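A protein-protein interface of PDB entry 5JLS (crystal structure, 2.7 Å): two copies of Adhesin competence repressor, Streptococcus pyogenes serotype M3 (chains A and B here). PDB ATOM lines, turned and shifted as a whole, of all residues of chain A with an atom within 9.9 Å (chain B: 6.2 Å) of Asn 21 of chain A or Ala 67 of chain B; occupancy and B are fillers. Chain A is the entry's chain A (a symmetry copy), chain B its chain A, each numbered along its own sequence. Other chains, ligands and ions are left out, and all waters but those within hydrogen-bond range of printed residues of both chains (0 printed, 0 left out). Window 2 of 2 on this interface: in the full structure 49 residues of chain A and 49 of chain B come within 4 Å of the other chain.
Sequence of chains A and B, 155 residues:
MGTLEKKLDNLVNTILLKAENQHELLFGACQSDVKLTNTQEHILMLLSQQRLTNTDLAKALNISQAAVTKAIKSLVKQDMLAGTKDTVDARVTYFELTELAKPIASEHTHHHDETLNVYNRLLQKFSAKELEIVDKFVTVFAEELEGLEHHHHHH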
ATOM      1  N   ASN A  13       3.122 -30.739 -11.491  1.00  0.00           N
ATOM      2  CA  ASN A  13       4.206 -30.135 -12.239  1.00  0.00           C
ATOM      3  C   ASN A  13       4.001 -30.217 -13.738  1.00  0.00           C
ATOM      4  O   ASN A  13       4.290 -29.258 -14.432  1.00  0.00           O
ATOM      5  CB  ASN A  13       5.555 -30.769 -11.877  1.00  0.00           C
ATOM      6  CG  ASN A  13       6.098 -30.279 -10.571  1.00  0.00           C
ATOM      7  OD1 ASN A  13       5.581 -29.328  -9.983  1.00  0.00           O
ATOM      8  ND2 ASN A  13       7.157 -30.938 -10.088  1.00  0.00           N
ATOM      9  N   THR A  14       3.486 -31.336 -14.237  1.00  0.00           N
ATOM     10  CA  THR A  14       3.232 -31.431 -15.656  1.00  0.00           C
ATOM     11  C   THR A  14       2.030 -30.599 -15.978  1.00  0.00           C
ATOM     12  O   THR A  14       2.034 -29.825 -16.934  1.00  0.00           O
ATOM     13  CB  THR A  14       3.079 -32.866 -16.186  1.00  0.00           C
ATOM     14  OG1 THR A  14       1.787 -33.392 -15.856  1.00  0.00           O
ATOM     15  CG2 THR A  14       4.227 -33.747 -15.662  1.00  0.00           C
ATOM     16  N   ILE A  15       1.009 -30.683 -15.153  1.00  0.00           N
ATOM     17  CA  ILE A  15      -0.097 -29.823 -15.408  1.00  0.00           C
ATOM     18  C   ILE A  15       0.386 -28.372 -15.568  1.00  0.00           C
ATOM     19  O   ILE A  15      -0.053 -27.690 -16.481  1.00  0.00           O
ATOM     20  CB  ILE A  15      -1.186 -29.986 -14.360  1.00  0.00           C
ATOM     21  CG1 ILE A  15      -1.860 -31.350 -14.541  1.00  0.00           C
ATOM     22  CG2 ILE A  15      -2.214 -28.853 -14.493  1.00  0.00           C
ATOM     23  CD1 ILE A  15      -2.569 -31.850 -13.303  1.00  0.00           C
ATOM     24  N   LEU A  16       1.291 -27.893 -14.733  1.00  0.00           N
ATOM     25  CA  LEU A  16       1.691 -26.455 -14.853  1.00  0.00           C
ATOM     26  C   LEU A  16       2.605 -26.167 -16.053  1.00  0.00           C
ATOM     27  O   LEU A  16       2.473 -25.133 -16.751  1.00  0.00           O
ATOM     28  CB  LEU A  16       2.402 -25.968 -13.608  1.00  0.00           C
ATOM     29  CG  LEU A  16       1.608 -26.073 -12.305  1.00  0.00           C
ATOM     30  CD1 LEU A  16       2.470 -25.797 -11.071  1.00  0.00           C
ATOM     31  CD2 LEU A  16       0.450 -25.123 -12.393  1.00  0.00           C
ATOM     32  N   LEU A  17       3.544 -27.080 -16.263  1.00  0.00           N
ATOM     33  CA  LEU A  17       4.575 -26.925 -17.290  1.00  0.00           C
ATOM     34  C   LEU A  17       4.015 -27.214 -18.670  1.00  0.00           C
ATOM     35  O   LEU A  17       4.414 -26.587 -19.633  1.00  0.00           O
ATOM     36  CB  LEU A  17       5.815 -27.771 -16.993  1.00  0.00           C
ATOM     37  CG  LEU A  17       6.590 -27.388 -15.724  1.00  0.00           C
ATOM     38  CD1 LEU A  17       7.914 -28.146 -15.623  1.00  0.00           C
ATOM     39  CD2 LEU A  17       6.820 -25.892 -15.600  1.00  0.00           C
ATOM     40  N   LYS A  18       3.032 -28.091 -18.767  1.00  0.00           N
ATOM     41  CA  LYS A  18       2.341 -28.276 -20.032  1.00  0.00           C
ATOM     42  C   LYS A  18       1.490 -27.046 -20.396  1.00  0.00           C
ATOM     43  O   LYS A  18       1.524 -26.619 -21.558  1.00  0.00           O
ATOM     44  CB  LYS A  18       1.522 -29.558 -20.026  1.00  0.00           C
ATOM     45  CG  LYS A  18       2.361 -30.830 -19.819  1.00  0.00           C
ATOM     46  CD  LYS A  18       3.092 -31.302 -21.066  1.00  0.00           C
ATOM     47  CE  LYS A  18       3.833 -32.605 -20.807  1.00  0.00           C
ATOM     48  NZ  LYS A  18       4.512 -33.137 -22.028  1.00  0.00           N
ATOM     49  N   ALA A  19       0.758 -26.462 -19.431  1.00  0.00           N
ATOM     50  CA  ALA A  19      -0.019 -25.248 -19.718  1.00  0.00           C
ATOM     51  C   ALA A  19       0.935 -24.171 -20.181  1.00  0.00           C
ATOM     52  O   ALA A  19       0.811 -23.718 -21.317  1.00  0.00           O
ATOM     53  CB  ALA A  19      -0.827 -24.767 -18.520  1.00  0.00           C
ATOM     54  N   GLU A  20       1.915 -23.818 -19.340  1.00  0.00           N
ATOM     55  CA  GLU A  20       2.893 -22.742 -19.667  1.00  0.00           C
ATOM     56  C   GLU A  20       3.457 -22.759 -21.089  1.00  0.00           C
ATOM     57  O   GLU A  20       3.484 -21.725 -21.748  1.00  0.00           O
ATOM     58  CB  GLU A  20       4.088 -22.761 -18.720  1.00  0.00           C
ATOM     59  CG  GLU A  20       3.848 -22.145 -17.365  1.00  0.00           C
ATOM     60  CD  GLU A  20       5.120 -21.992 -16.575  1.00  0.00           C
ATOM     61  OE1 GLU A  20       5.047 -21.396 -15.497  1.00  0.00           O
ATOM     62  OE2 GLU A  20       6.210 -22.413 -17.030  1.00  0.00           O
ATOM     63  N   ASN A  21       3.884 -23.932 -21.546  1.00  0.00           N
ATOM     64  CA  ASN A  21       4.755 -24.050 -22.723  1.00  0.00           C
ATOM     65  C   ASN A  21       3.952 -24.437 -23.966  1.00  0.00           C
ATOM     66  O   ASN A  21       3.882 -23.649 -24.917  1.00  0.00           O
ATOM     67  CB  ASN A  21       5.949 -25.011 -22.448  1.00  0.00           C
ATOM     68  CG  ASN A  21       6.945 -24.448 -21.401  1.00  0.00           C
ATOM     69  OD1 ASN A  21       7.676 -23.477 -21.661  1.00  0.00           O
ATOM     70  ND2 ASN A  21       6.976 -25.064 -20.212  1.00  0.00           N
ATOM     71  N   GLN A  22       3.369 -25.637 -23.950  1.00  0.00           N
ATOM     72  CA  GLN A  22       2.354 -26.060 -24.929  1.00  0.00           C
ATOM     73  C   GLN A  22       2.876 -26.185 -26.384  1.00  0.00           C
ATOM     74  O   GLN A  22       2.593 -27.157 -27.109  1.00  0.00           O
ATOM     75  CB  GLN A  22       1.120 -25.133 -24.832  1.00  0.00           C
ATOM     76  CG  GLN A  22       1.091 -23.936 -25.778  1.00  0.00           C
ATOM     77  CD  GLN A  22       0.502 -22.696 -25.144  1.00  0.00           C
ATOM     78  OE1 GLN A  22      -0.544 -22.755 -24.494  1.00  0.00           O
ATOM     79  NE2 GLN A  22       1.165 -21.559 -25.337  1.00  0.00           N
ATOM     80  N   ASN A  38      -5.124 -18.233 -18.194  1.00  0.00           N
ATOM     81  CA  ASN A  38      -6.211 -19.149 -17.944  1.00  0.00           C
ATOM     82  C   ASN A  38      -7.363 -18.542 -17.193  1.00  0.00           C
ATOM     83  O   ASN A  38      -8.519 -18.865 -17.477  1.00  0.00           O
ATOM     84  CB  ASN A  38      -5.704 -20.408 -17.244  1.00  0.00           C
ATOM     85  CG  ASN A  38      -5.089 -21.380 -18.235  1.00  0.00           C
ATOM     86  OD1 ASN A  38      -5.777 -21.853 -19.127  1.00  0.00           O
ATOM     87  ND2 ASN A  38      -3.803 -21.630 -18.119  1.00  0.00           N
ATOM     88  N   THR B  37       8.859 -18.124 -14.659  1.00  0.00           N
ATOM     89  CA  THR B  37       7.907 -19.194 -14.935  1.00  0.00           C
ATOM     90  C   THR B  37       8.160 -20.379 -13.995  1.00  0.00           C
ATOM     91  O   THR B  37       9.190 -20.449 -13.320  1.00  0.00           O
ATOM     92  CB  THR B  37       7.956 -19.662 -16.413  1.00  0.00           C
ATOM     93  OG1 THR B  37       9.196 -20.340 -16.704  1.00  0.00           O
ATOM     94  CG2 THR B  37       7.742 -18.475 -17.355  1.00  0.00           C
ATOM     95  N   THR B  39       8.539 -23.331 -15.329  1.00  0.00           N
ATOM     96  CA  THR B  39       9.583 -23.910 -16.130  1.00  0.00           C
ATOM     97  C   THR B  39      10.920 -23.387 -15.659  1.00  0.00           C
ATOM     98  O   THR B  39      11.847 -24.157 -15.372  1.00  0.00           O
ATOM     99  CB  THR B  39       9.438 -23.493 -17.578  1.00  0.00           C
ATOM    100  OG1 THR B  39       8.063 -23.601 -17.955  1.00  0.00           O
ATOM    101  CG2 THR B  39      10.329 -24.363 -18.473  1.00  0.00           C
ATOM    102  N   ILE B  43      13.796 -25.472 -13.751  1.00  0.00           N
ATOM    103  CA  ILE B  43      15.043 -25.585 -14.437  1.00  0.00           C
ATOM    104  C   ILE B  43      16.082 -25.242 -13.353  1.00  0.00           C
ATOM    105  O   ILE B  43      17.058 -25.983 -13.154  1.00  0.00           O
ATOM    106  CB  ILE B  43      15.096 -24.621 -15.678  1.00  0.00           C
ATOM    107  CG1 ILE B  43      14.479 -25.302 -16.904  1.00  0.00           C
ATOM    108  CG2 ILE B  43      16.536 -24.188 -15.999  1.00  0.00           C
ATOM    109  CD1 ILE B  43      14.245 -24.400 -18.108  1.00  0.00           C
ATOM    110  N   ILE B  63       9.295 -31.538 -21.644  1.00  0.00           N
ATOM    111  CA  ILE B  63       8.923 -30.363 -22.467  1.00  0.00           C
ATOM    112  C   ILE B  63       9.834 -30.293 -23.687  1.00  0.00           C
ATOM    113  O   ILE B  63      10.861 -31.007 -23.760  1.00  0.00           O
ATOM    114  CB  ILE B  63       8.965 -28.993 -21.694  1.00  0.00           C
ATOM    115  CG1 ILE B  63      10.274 -28.810 -20.892  1.00  0.00           C
ATOM    116  CG2 ILE B  63       7.775 -28.832 -20.747  1.00  0.00           C
ATOM    117  CD1 ILE B  63      10.374 -27.494 -20.139  1.00  0.00           C
ATOM    118  N   SER B  64       9.456 -29.435 -24.641  1.00  0.00           N
ATOM    119  CA  SER B  64      10.245 -29.232 -25.864  1.00  0.00           C
ATOM    120  C   SER B  64      11.603 -28.616 -25.521  1.00  0.00           C
ATOM    121  O   SER B  64      11.741 -27.842 -24.522  1.00  0.00           O
ATOM    122  CB  SER B  64       9.517 -28.351 -26.884  1.00  0.00           C
ATOM    123  OG  SER B  64       9.140 -27.099 -26.327  1.00  0.00           O
ATOM    124  N   GLN B  65      12.584 -29.025 -26.335  1.00  0.00           N
ATOM    125  CA  GLN B  65      13.909 -28.439 -26.386  1.00  0.00           C
ATOM    126  C   GLN B  65      13.785 -26.929 -26.479  1.00  0.00           C
ATOM    127  O   GLN B  65      14.434 -26.176 -25.731  1.00  0.00           O
ATOM    128  CB  GLN B  65      14.628 -28.938 -27.643  1.00  0.00           C
ATOM    129  CG  GLN B  65      16.138 -28.824 -27.587  1.00  0.00           C
ATOM    130  CD  GLN B  65      16.750 -29.955 -26.781  1.00  0.00           C
ATOM    131  OE1 GLN B  65      16.434 -31.136 -26.984  1.00  0.00           O
ATOM    132  NE2 GLN B  65      17.619 -29.602 -25.859  1.00  0.00           N
ATOM    133  N   ALA B  66      12.921 -26.515 -27.407  1.00  0.00           N
ATOM    134  CA  ALA B  66      12.656 -25.111 -27.709  1.00  0.00           C
ATOM    135  C   ALA B  66      12.142 -24.309 -26.503  1.00  0.00           C
ATOM    136  O   ALA B  66      12.452 -23.117 -26.320  1.00  0.00           O
ATOM    137  CB  ALA B  66      11.653 -25.020 -28.853  1.00  0.00           C
ATOM    138  N   ALA B  67      11.326 -24.966 -25.695  1.00  0.00           N
ATOM    139  CA  ALA B  67      10.791 -24.351 -24.511  1.00  0.00           C
ATOM    140  C   ALA B  67      11.895 -24.144 -23.474  1.00  0.00           C
ATOM    141  O   ALA B  67      11.875 -23.152 -22.720  1.00  0.00           O
ATOM    142  CB  ALA B  67       9.620 -25.168 -23.966  1.00  0.00           C
ATOM    143  N   VAL B  68      12.873 -25.052 -23.441  1.00  0.00           N
ATOM    144  CA  VAL B  68      14.006 -24.929 -22.487  1.00  0.00           C
ATOM    145  C   VAL B  68      14.869 -23.745 -22.948  1.00  0.00           C
ATOM    146  O   VAL B  68      15.145 -22.825 -22.190  1.00  0.00           O
ATOM    147  CB  VAL B  68      14.844 -26.230 -22.354  1.00  0.00           C
ATOM    148  CG1 VAL B  68      15.977 -26.047 -21.336  1.00  0.00           C
ATOM    149  CG2 VAL B  68      13.959 -27.441 -22.042  1.00  0.00           C
ATOM    150  N   THR B  69      15.209 -23.750 -24.224  1.00  0.00           N
ATOM    151  CA  THR B  69      15.973 -22.666 -24.803  1.00  0.00           C
ATOM    152  C   THR B  69      15.271 -21.292 -24.650  1.00  0.00           C
ATOM    153  O   THR B  69      15.962 -20.280 -24.568  1.00  0.00           O
ATOM    154  CB  THR B  69      16.271 -22.935 -26.283  1.00  0.00           C
ATOM    155  OG1 THR B  69      15.063 -23.333 -26.911  1.00  0.00           O
ATOM    156  CG2 THR B  69      17.226 -24.041 -26.459  1.00  0.00           C
ATOM    157  N   LYS B  70      13.940 -21.228 -24.608  1.00  0.00           N
ATOM    158  CA  LYS B  70      13.264 -19.902 -24.353  1.00  0.00           C
ATOM    159  C   LYS B  70      13.632 -19.462 -22.920  1.00  0.00           C
ATOM    160  O   LYS B  70      14.309 -18.442 -22.703  1.00  0.00           O
ATOM    161  CB  LYS B  70      11.724 -19.961 -24.622  1.00  0.00           C
ATOM    162  CG  LYS B  70      10.775 -19.056 -23.790  1.00  0.00           C
ATOM    163  CD  LYS B  70      11.109 -17.547 -23.686  1.00  0.00           C
ATOM    164  CE  LYS B  70      11.362 -16.877 -25.025  1.00  0.00           C
ATOM    165  NZ  LYS B  70      10.224 -17.117 -25.955  1.00  0.00           N
ATOM    166  N   ALA B  71      13.216 -20.316 -21.978  1.00  0.00           N
ATOM    167  CA  ALA B  71      13.408 -20.173 -20.541  1.00  0.00           C
ATOM    168  C   ALA B  71      14.862 -19.895 -20.166  1.00  0.00           C
ATOM    169  O   ALA B  71      15.146 -18.966 -19.357  1.00  0.00           O
ATOM    170  CB  ALA B  71      12.924 -21.438 -19.861  1.00  0.00           C
ATOM    171  N   ILE B  72      15.757 -20.678 -20.784  1.00  0.00           N
ATOM    172  CA  ILE B  72      17.207 -20.563 -20.581  1.00  0.00           C
ATOM    173  C   ILE B  72      17.729 -19.191 -20.908  1.00  0.00           C
ATOM    174  O   ILE B  72      18.512 -18.624 -20.131  1.00  0.00           O
ATOM    175  CB  ILE B  72      18.032 -21.600 -21.399  1.00  0.00           C
ATOM    176  CG1 ILE B  72      17.814 -23.044 -20.867  1.00  0.00           C
ATOM    177  CG2 ILE B  72      19.552 -21.269 -21.341  1.00  0.00           C
ATOM    178  CD1 ILE B  72      18.465 -23.299 -19.531  1.00  0.00           C
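OG1 of Thr 39 of chain B lies within hydrogen-bond range of ND2 of Asn 21 of chain A.
The backbone NH (N) of Thr 39 of chain B sits at hydrogen-bond distance from the side-chain carboxylate (OE2) of Glu 20 of chain A, 3.0 Å away.
The backbone NH of Thr 39 of chain B sits close to the side-chain hydroxyl of Thr 37 of chain B, at 3.4 Å.
The side-chain hydroxyl of Ser 64 of chain B sits close to the backbone NH of Ala 67 of chain B (3.1 Å).
The side-chain amide nitrogen (ND2) of Asn 21 of chain A sits at hydrogen-bond distance from the backbone carbonyl oxygen (O) of Leu 17 of chain A, at 3.0 Å.
Leu 17 of chain A touches Thr 39 of chain B (CD2 to N, 3.1 Å).
Glu 20 of chain A touches Thr 37 of chain B.
ND2 of Asn 21 of chain A touches CG2 of Ile 63 of chain B (3.9 Å).
Ala 67 of chain B touches Asn 21 of chain A.
Of the printed residues of chain B, Leu 17 of chain A touches Thr 39.
Of the printed residues of chain B, Glu 20 of chain A touches Thr 37 (3.3 Å) and Thr 39 (2.4 Å).
Asn 21 of chain A touches just these residues of chain B: Thr 39 (2.9 Å), Ile 63 (3.9 Å) and Ala 67 (3.5 Å).
Of the printed residues of chain A, Thr 37 of chain B touches Glu 20.
Ile 43 of chain B touches none of the printed residues of chain A.
No residue of chain A comes within 4 Å of Ser 64 of chain B.
Ala 66 of chain B touches none of the printed residues of chain A.
Of chain A, only Asn 21 comes within 4 Å of Ala 67 of chain B.
No residue of chain A comes within 4 Å of Val 68 of chain B.
Lys 70 of chain B touches none of the printed residues of chain A.
The nearest residue of chain B that does not touch Asn 21 of chain A is Ser 64 of chain B (5.4 Å).
The nearest residue of chain A that does not touch Ala 67 of chain B is Gln 22 of chain A (6.3 Å).
The nearest printed residue of chain B that does not touch Glu 20 of chain A is Ala 67 of chain B (7.2 Å).
Of the 11 printed residues of chain A, 3 touch a printed residue of chain B.
Printed residues of chain A that touch a printed residue of chain B: Leu 17, Glu 20 and Asn 21.
Hydrophobic or aromatic side chains of chain A within 4 Å of the printed part of chain B: Leu 17.
Along chain A the printed residues that touch a printed residue of chain B span positions 17 to 21.
Printed residues of chain B that touch a printed residue of chain A: Thr 37, Thr 39, Ile 63 and Ala 67.
Hydrophobic or aromatic side chains of chain B within 4 Å of the printed part of chain A: Ile 63 and Ala 67.
Among the printed residues, 6 pairs touch across the chains.
Among the printed residues, no Asp or Glu carboxylate lies within 4 Å of a Lys or Arg side-chain nitrogen of the other chain.
No position is printed for both chains.
Of the 6 pairs that touch across the chains among the printed residues, none has its exchanged pair printed and touching as well.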
